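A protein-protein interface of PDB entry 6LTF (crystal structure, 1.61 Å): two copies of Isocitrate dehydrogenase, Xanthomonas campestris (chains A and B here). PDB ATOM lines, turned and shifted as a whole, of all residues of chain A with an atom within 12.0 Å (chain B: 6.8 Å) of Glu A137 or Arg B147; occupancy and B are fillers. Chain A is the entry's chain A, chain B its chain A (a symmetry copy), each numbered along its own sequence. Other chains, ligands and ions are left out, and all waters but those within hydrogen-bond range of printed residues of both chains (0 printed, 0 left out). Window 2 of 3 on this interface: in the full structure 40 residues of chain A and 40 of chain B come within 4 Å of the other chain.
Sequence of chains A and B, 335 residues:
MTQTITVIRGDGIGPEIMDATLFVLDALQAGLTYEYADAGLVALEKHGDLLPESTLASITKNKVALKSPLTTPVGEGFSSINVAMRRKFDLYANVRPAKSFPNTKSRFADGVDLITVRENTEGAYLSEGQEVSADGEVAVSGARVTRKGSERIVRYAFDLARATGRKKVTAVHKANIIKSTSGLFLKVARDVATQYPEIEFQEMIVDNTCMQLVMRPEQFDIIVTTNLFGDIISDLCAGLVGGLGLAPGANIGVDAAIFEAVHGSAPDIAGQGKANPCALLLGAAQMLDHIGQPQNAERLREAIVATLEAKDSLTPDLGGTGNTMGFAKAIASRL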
ATOM      1  N   GLU A 131      23.339 -30.002   0.683  1.00  0.00           N
ATOM      2  CA  GLU A 131      22.724 -31.143   0.015  1.00  0.00           C
ATOM      3  C   GLU A 131      21.280 -30.825  -0.349  1.00  0.00           C
ATOM      4  O   GLU A 131      20.597 -30.081   0.361  1.00  0.00           O
ATOM      5  CB  GLU A 131      22.792 -32.416   0.882  1.00  0.00           C
ATOM      6  CG  GLU A 131      22.360 -33.682   0.107  1.00  0.00           C
ATOM      7  CD  GLU A 131      22.973 -34.971   0.636  1.00  0.00           C
ATOM      8  OE1 GLU A 131      22.657 -36.041   0.066  1.00  0.00           O
ATOM      9  OE2 GLU A 131      23.760 -34.920   1.604  1.00  0.00           O
ATOM     10  N   VAL A 132      20.827 -31.378  -1.469  1.00  0.00           N
ATOM     11  CA  VAL A 132      19.420 -31.343  -1.860  1.00  0.00           C
ATOM     12  C   VAL A 132      18.902 -32.774  -1.848  1.00  0.00           C
ATOM     13  O   VAL A 132      19.571 -33.687  -2.355  1.00  0.00           O
ATOM     14  CB  VAL A 132      19.220 -30.701  -3.247  1.00  0.00           C
ATOM     15  CG1 VAL A 132      17.732 -30.521  -3.527  1.00  0.00           C
ATOM     16  CG2 VAL A 132      19.955 -29.371  -3.336  1.00  0.00           C
ATOM     17  N   SER A 133      17.721 -32.972  -1.266  1.00  0.00           N
ATOM     18  CA  SER A 133      17.113 -34.298  -1.253  1.00  0.00           C
ATOM     19  C   SER A 133      16.855 -34.786  -2.677  1.00  0.00           C
ATOM     20  O   SER A 133      16.710 -33.994  -3.611  1.00  0.00           O
ATOM     21  CB  SER A 133      15.806 -34.263  -0.463  1.00  0.00           C
ATOM     22  OG  SER A 133      14.821 -33.484  -1.122  1.00  0.00           O
ATOM     23  N   ALA A 134      16.778 -36.117  -2.831  1.00  0.00           N
ATOM     24  CA  ALA A 134      16.611 -36.710  -4.157  1.00  0.00           C
ATOM     25  C   ALA A 134      15.344 -36.213  -4.846  1.00  0.00           C
ATOM     26  O   ALA A 134      15.350 -35.973  -6.062  1.00  0.00           O
ATOM     27  CB  ALA A 134      16.602 -38.236  -4.058  1.00  0.00           C
ATOM     28  N   ASP A 135      14.248 -36.043  -4.092  1.00  0.00           N
ATOM     29  CA  ASP A 135      13.005 -35.587  -4.708  1.00  0.00           C
ATOM     30  C   ASP A 135      12.975 -34.083  -4.960  1.00  0.00           C
ATOM     31  O   ASP A 135      11.984 -33.585  -5.504  1.00  0.00           O
ATOM     32  CB  ASP A 135      11.788 -36.002  -3.869  1.00  0.00           C
ATOM     33  CG  ASP A 135      11.790 -35.425  -2.450  1.00  0.00           C
ATOM     34  OD1 ASP A 135      12.556 -34.487  -2.145  1.00  0.00           O
ATOM     35  OD2 ASP A 135      10.989 -35.917  -1.632  1.00  0.00           O
ATOM     36  N   GLY A 136      14.032 -33.359  -4.591  1.00  0.00           N
ATOM     37  CA  GLY A 136      14.120 -31.945  -4.882  1.00  0.00           C
ATOM     38  C   GLY A 136      13.331 -31.043  -3.964  1.00  0.00           C
ATOM     39  O   GLY A 136      13.279 -29.833  -4.218  1.00  0.00           O
ATOM     40  N   GLU A 137      12.732 -31.580  -2.895  1.00  0.00           N
ATOM     41  CA  GLU A 137      11.838 -30.784  -2.057  1.00  0.00           C
ATOM     42  C   GLU A 137      12.579 -29.996  -0.982  1.00  0.00           C
ATOM     43  O   GLU A 137      12.124 -28.912  -0.596  1.00  0.00           O
ATOM     44  CB  GLU A 137      10.791 -31.684  -1.399  1.00  0.00           C
ATOM     45  CG  GLU A 137       9.875 -30.955  -0.413  1.00  0.00           C
ATOM     46  CD  GLU A 137       9.054 -29.867  -1.078  1.00  0.00           C
ATOM     47  OE1 GLU A 137       8.481 -30.152  -2.174  1.00  0.00           O
ATOM     48  OE2 GLU A 137       9.001 -28.733  -0.507  1.00  0.00           O
ATOM     49  N   VAL A 138      13.694 -30.521  -0.469  1.00  0.00           N
ATOM     50  CA  VAL A 138      14.348 -29.958   0.712  1.00  0.00           C
ATOM     51  C   VAL A 138      15.838 -29.767   0.447  1.00  0.00           C
ATOM     52  O   VAL A 138      16.550 -30.731   0.124  1.00  0.00           O
ATOM     53  CB  VAL A 138      14.138 -30.845   1.951  1.00  0.00           C
ATOM     54  CG1 VAL A 138      14.864 -30.257   3.139  1.00  0.00           C
ATOM     55  CG2 VAL A 138      12.645 -31.000   2.269  1.00  0.00           C
ATOM     56  N   ALA A 139      16.316 -28.528   0.626  1.00  0.00           N
ATOM     57  CA  ALA A 139      17.735 -28.193   0.576  1.00  0.00           C
ATOM     58  C   ALA A 139      18.235 -27.746   1.946  1.00  0.00           C
ATOM     59  O   ALA A 139      17.518 -27.067   2.690  1.00  0.00           O
ATOM     60  CB  ALA A 139      17.997 -27.076  -0.441  1.00  0.00           C
ATOM     61  N   VAL A 140      19.467 -28.137   2.271  1.00  0.00           N
ATOM     62  CA  VAL A 140      20.120 -27.717   3.504  1.00  0.00           C
ATOM     63  C   VAL A 140      21.503 -27.183   3.169  1.00  0.00           C
ATOM     64  O   VAL A 140      22.147 -27.611   2.198  1.00  0.00           O
ATOM     65  CB  VAL A 140      20.198 -28.871   4.538  1.00  0.00           C
ATOM     66  CG1 VAL A 140      18.779 -29.345   4.927  1.00  0.00           C
ATOM     67  CG2 VAL A 140      21.074 -30.025   4.016  1.00  0.00           C
ATOM     68  N   SER A 141      21.933 -26.209   3.971  1.00  0.00           N
ATOM     69  CA  SER A 141      23.300 -25.717   3.974  1.00  0.00           C
ATOM     70  C   SER A 141      23.661 -25.414   5.419  1.00  0.00           C
ATOM     71  O   SER A 141      22.799 -25.375   6.295  1.00  0.00           O
ATOM     72  CB  SER A 141      23.481 -24.493   3.049  1.00  0.00           C
ATOM     73  OG  SER A 141      22.692 -23.390   3.458  1.00  0.00           O
ATOM     74  N   GLU B 122      11.715 -19.890   6.973  1.00  0.00           N
ATOM     75  CA  GLU B 122      12.834 -20.836   6.877  1.00  0.00           C
ATOM     76  C   GLU B 122      14.134 -20.085   6.573  1.00  0.00           C
ATOM     77  O   GLU B 122      14.354 -19.002   7.124  1.00  0.00           O
ATOM     78  CB  GLU B 122      12.522 -21.936   5.840  1.00  0.00           C
ATOM     79  CG  GLU B 122      12.107 -21.430   4.448  1.00  0.00           C
ATOM     80  CD  GLU B 122      11.708 -22.544   3.476  1.00  0.00           C
ATOM     81  OE1 GLU B 122      11.104 -23.572   3.913  1.00  0.00           O
ATOM     82  OE2 GLU B 122      11.981 -22.382   2.261  1.00  0.00           O
ATOM     83  N   VAL B 145      16.009 -24.536   2.936  1.00  0.00           N
ATOM     84  CA  VAL B 145      15.140 -23.916   1.937  1.00  0.00           C
ATOM     85  C   VAL B 145      14.337 -25.044   1.300  1.00  0.00           C
ATOM     86  O   VAL B 145      14.904 -26.088   0.957  1.00  0.00           O
ATOM     87  CB  VAL B 145      15.942 -23.127   0.883  1.00  0.00           C
ATOM     88  CG1 VAL B 145      15.044 -22.692  -0.269  1.00  0.00           C
ATOM     89  CG2 VAL B 145      16.592 -21.904   1.525  1.00  0.00           C
ATOM     90  N   THR B 146      13.030 -24.853   1.178  1.00  0.00           N
ATOM     91  CA  THR B 146      12.189 -25.878   0.572  1.00  0.00           C
ATOM     92  C   THR B 146      11.523 -25.359  -0.694  1.00  0.00           C
ATOM     93  O   THR B 146      11.346 -24.144  -0.898  1.00  0.00           O
ATOM     94  CB  THR B 146      11.123 -26.397   1.549  1.00  0.00           C
ATOM     95  OG1 THR B 146      10.230 -25.341   1.923  1.00  0.00           O
ATOM     96  CG2 THR B 146      11.775 -26.974   2.813  1.00  0.00           C
ATOM     97  N   ARG B 147      11.165 -26.316  -1.557  1.00  0.00           N
ATOM     98  CA  ARG B 147      10.377 -25.978  -2.728  1.00  0.00           C
ATOM     99  C   ARG B 147       9.060 -25.321  -2.324  1.00  0.00           C
ATOM    100  O   ARG B 147       8.672 -24.300  -2.899  1.00  0.00           O
ATOM    101  CB  ARG B 147      10.132 -27.218  -3.586  1.00  0.00           C
ATOM    102  CG  ARG B 147       9.399 -26.901  -4.877  1.00  0.00           C
ATOM    103  CD  ARG B 147       8.566 -28.091  -5.329  1.00  0.00           C
ATOM    104  NE  ARG B 147       7.744 -28.613  -4.233  1.00  0.00           N
ATOM    105  CZ  ARG B 147       6.595 -28.082  -3.815  1.00  0.00           C
ATOM    106  NH1 ARG B 147       6.095 -26.992  -4.395  1.00  0.00           N
ATOM    107  NH2 ARG B 147       5.942 -28.645  -2.803  1.00  0.00           N
ATOM    108  N   LYS B 148       8.369 -25.874  -1.321  1.00  0.00           N
ATOM    109  CA  LYS B 148       7.087 -25.310  -0.888  1.00  0.00           C
ATOM    110  C   LYS B 148       7.258 -23.886  -0.362  1.00  0.00           C
ATOM    111  O   LYS B 148       6.527 -22.960  -0.754  1.00  0.00           O
ATOM    112  CB  LYS B 148       6.464 -26.227   0.173  1.00  0.00           C
ATOM    113  CG  LYS B 148       5.130 -25.773   0.777  1.00  0.00           C
ATOM    114  CD  LYS B 148       4.805 -26.641   2.009  1.00  0.00           C
ATOM    115  CE  LYS B 148       3.401 -26.382   2.579  1.00  0.00           C
ATOM    116  NZ  LYS B 148       3.140 -24.953   2.897  1.00  0.00           N
ATOM    117  N   GLY B 149       8.257 -23.677   0.496  1.00  0.00           N
ATOM    118  CA  GLY B 149       8.431 -22.351   1.076  1.00  0.00           C
ATOM    119  C   GLY B 149       8.878 -21.315   0.057  1.00  0.00           C
ATOM    120  O   GLY B 149       8.401 -20.162   0.065  1.00  0.00           O
ATOM    121  N   SER B 150       9.791 -21.707  -0.843  1.00  0.00           N
ATOM    122  CA  SER B 150      10.193 -20.813  -1.930  1.00  0.00           C
ATOM    123  C   SER B 150       9.033 -20.509  -2.874  1.00  0.00           C
ATOM    124  O   SER B 150       8.838 -19.354  -3.285  1.00  0.00           O
ATOM    125  CB  SER B 150      11.382 -21.408  -2.690  1.00  0.00           C
ATOM    126  OG  SER B 150      12.472 -21.602  -1.808  1.00  0.00           O
ATOM    127  N   GLU B 151       8.237 -21.526  -3.227  1.00  0.00           N
ATOM    128  CA  GLU B 151       7.146 -21.286  -4.160  1.00  0.00           C
ATOM    129  C   GLU B 151       6.167 -20.264  -3.592  1.00  0.00           C
ATOM    130  O   GLU B 151       5.734 -19.345  -4.306  1.00  0.00           O
ATOM    131  CB  GLU B 151       6.435 -22.597  -4.490  1.00  0.00           C
ATOM    132  CG  GLU B 151       5.330 -22.410  -5.511  1.00  0.00           C
ATOM    133  CD  GLU B 151       4.872 -23.720  -6.126  1.00  0.00           C
ATOM    134  OE1 GLU B 151       5.540 -24.751  -5.891  1.00  0.00           O
ATOM    135  OE2 GLU B 151       3.857 -23.712  -6.861  1.00  0.00           O
ATOM    136  N   ARG B 152       5.816 -20.385  -2.300  1.00  0.00           N
ATOM    137  CA  ARG B 152       4.796 -19.471  -1.790  1.00  0.00           C
ATOM    138  C   ARG B 152       5.326 -18.039  -1.660  1.00  0.00           C
ATOM    139  O   ARG B 152       4.590 -17.080  -1.943  1.00  0.00           O
ATOM    140  CB  ARG B 152       4.204 -19.986  -0.466  1.00  0.00           C
ATOM    141  CG  ARG B 152       5.152 -20.127   0.718  1.00  0.00           C
ATOM    142  CD  ARG B 152       4.374 -20.645   1.952  1.00  0.00           C
ATOM    143  NE  ARG B 152       5.201 -20.756   3.159  1.00  0.00           N
ATOM    144  CZ  ARG B 152       4.733 -21.117   4.351  1.00  0.00           C
ATOM    145  NH1 ARG B 152       3.452 -21.437   4.488  1.00  0.00           N
ATOM    146  NH2 ARG B 152       5.543 -21.197   5.401  1.00  0.00           N
ATOM    147  N   LEU B 184      18.232 -23.673  -4.856  1.00  0.00           N
ATOM    148  CA  LEU B 184      16.847 -24.146  -4.916  1.00  0.00           C
ATOM    149  C   LEU B 184      15.876 -22.971  -4.927  1.00  0.00           C
ATOM    150  O   LEU B 184      14.891 -22.971  -5.678  1.00  0.00           O
ATOM    151  CB  LEU B 184      16.551 -25.080  -3.739  1.00  0.00           C
ATOM    152  CG  LEU B 184      15.094 -25.569  -3.702  1.00  0.00           C
ATOM    153  CD1 LEU B 184      14.747 -26.337  -4.969  1.00  0.00           C
ATOM    154  CD2 LEU B 184      14.785 -26.393  -2.444  1.00  0.00           C
ATOM    155  N   VAL B 188      13.331 -22.312  -8.104  1.00  0.00           N
ATOM    156  CA  VAL B 188      11.892 -22.166  -7.917  1.00  0.00           C
ATOM    157  C   VAL B 188      11.419 -20.797  -8.399  1.00  0.00           C
ATOM    158  O   VAL B 188      10.368 -20.684  -9.040  1.00  0.00           O
ATOM    159  CB  VAL B 188      11.514 -22.412  -6.444  1.00  0.00           C
ATOM    160  CG1 VAL B 188      10.056 -22.006  -6.191  1.00  0.00           C
ATOM    161  CG2 VAL B 188      11.740 -23.871  -6.074  1.00  0.00           C
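NE of Arg B147 is in salt-bridge range of OE1 of Glu A137 (2.7 Å). OE2 of Glu A137 sits at hydrogen-bond distance from N of Lys B148 (3.0 Å). The backbone NH of Ala A139 sits at hydrogen-bond distance from the backbone carbonyl oxygen of Val B145 (2.8 Å).
The side-chain hydroxyl (OG) of Ser A133 is in hydrogen-bond range of the backbone NH (N) of Glu A137 (3.3 Å). The side-chain hydroxyl (OG1) of Thr B146 is in hydrogen-bond range of the side-chain carboxylate (OE1) of Glu B122 (2.8 Å). The backbone carbonyl oxygen (O) of Val A138 lies within hydrogen-bond range of the backbone NH (N) of Ser A133. OG1 of Thr B146 sits at hydrogen-bond distance from N of Gly B149, at 2.9 Å. The side-chain carboxylate (OD1) of Asp A135 sits at hydrogen-bond distance from the backbone NH (N) of Glu A137, at 3.0 Å. The side-chain carboxylate of Glu B151 is in salt-bridge range of the guanidinium group of Arg B147, at 2.8 Å.
Among the printed residues, merely in contact across the chains: Gly A136 with Leu B184 (3.9 Å), Glu A137 with Thr B146 (3.3 Å), Val A138 with Val B145 (3.8 Å) and Ala A139 with Leu B184 (3.8 Å).
Glu A137 touches just these residues of chain B: Thr B146 (3.3 Å), Arg B147 (2.7 Å) and Lys B148 (3.0 Å). Of the printed residues of chain B, Val A138 touches Val B145 (3.8 Å). Of the printed residues of chain B, Ala A139 touches Val B145 and Leu B184. Of chain A, only Val A138 and Ala A139 come within 4 Å of Val B145. Of chain A, only Glu A137 (2.7 Å) comes within 4 Å of Arg B147. Of chain A, only Glu A137 comes within 4 Å of Lys B148. No residue of chain A comes within 4 Å of Gly B149. No residue of chain A comes within 4 Å of Ser B150. No residue of chain A comes within 4 Å of Glu B151. No residue of chain A comes within 4 Å of Val B188. The nearest printed residue of chain B that does not touch Val A138 is Thr B146 (4.2 Å).
Of the 11 printed residues of chain B, 5 touch a printed residue of chain A. Along chain B the printed residues that touch a printed residue of chain A span positions 145 to 184. Among the printed residues, Asp or Glu carboxylates within 4 Å of a Lys or Arg side-chain nitrogen of the other chain: Glu A137 with Arg B147.
No position is printed for both chains. Of the 7 pairs that touch across the chains among the printed residues, none has its exchanged pair printed and touching as well.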
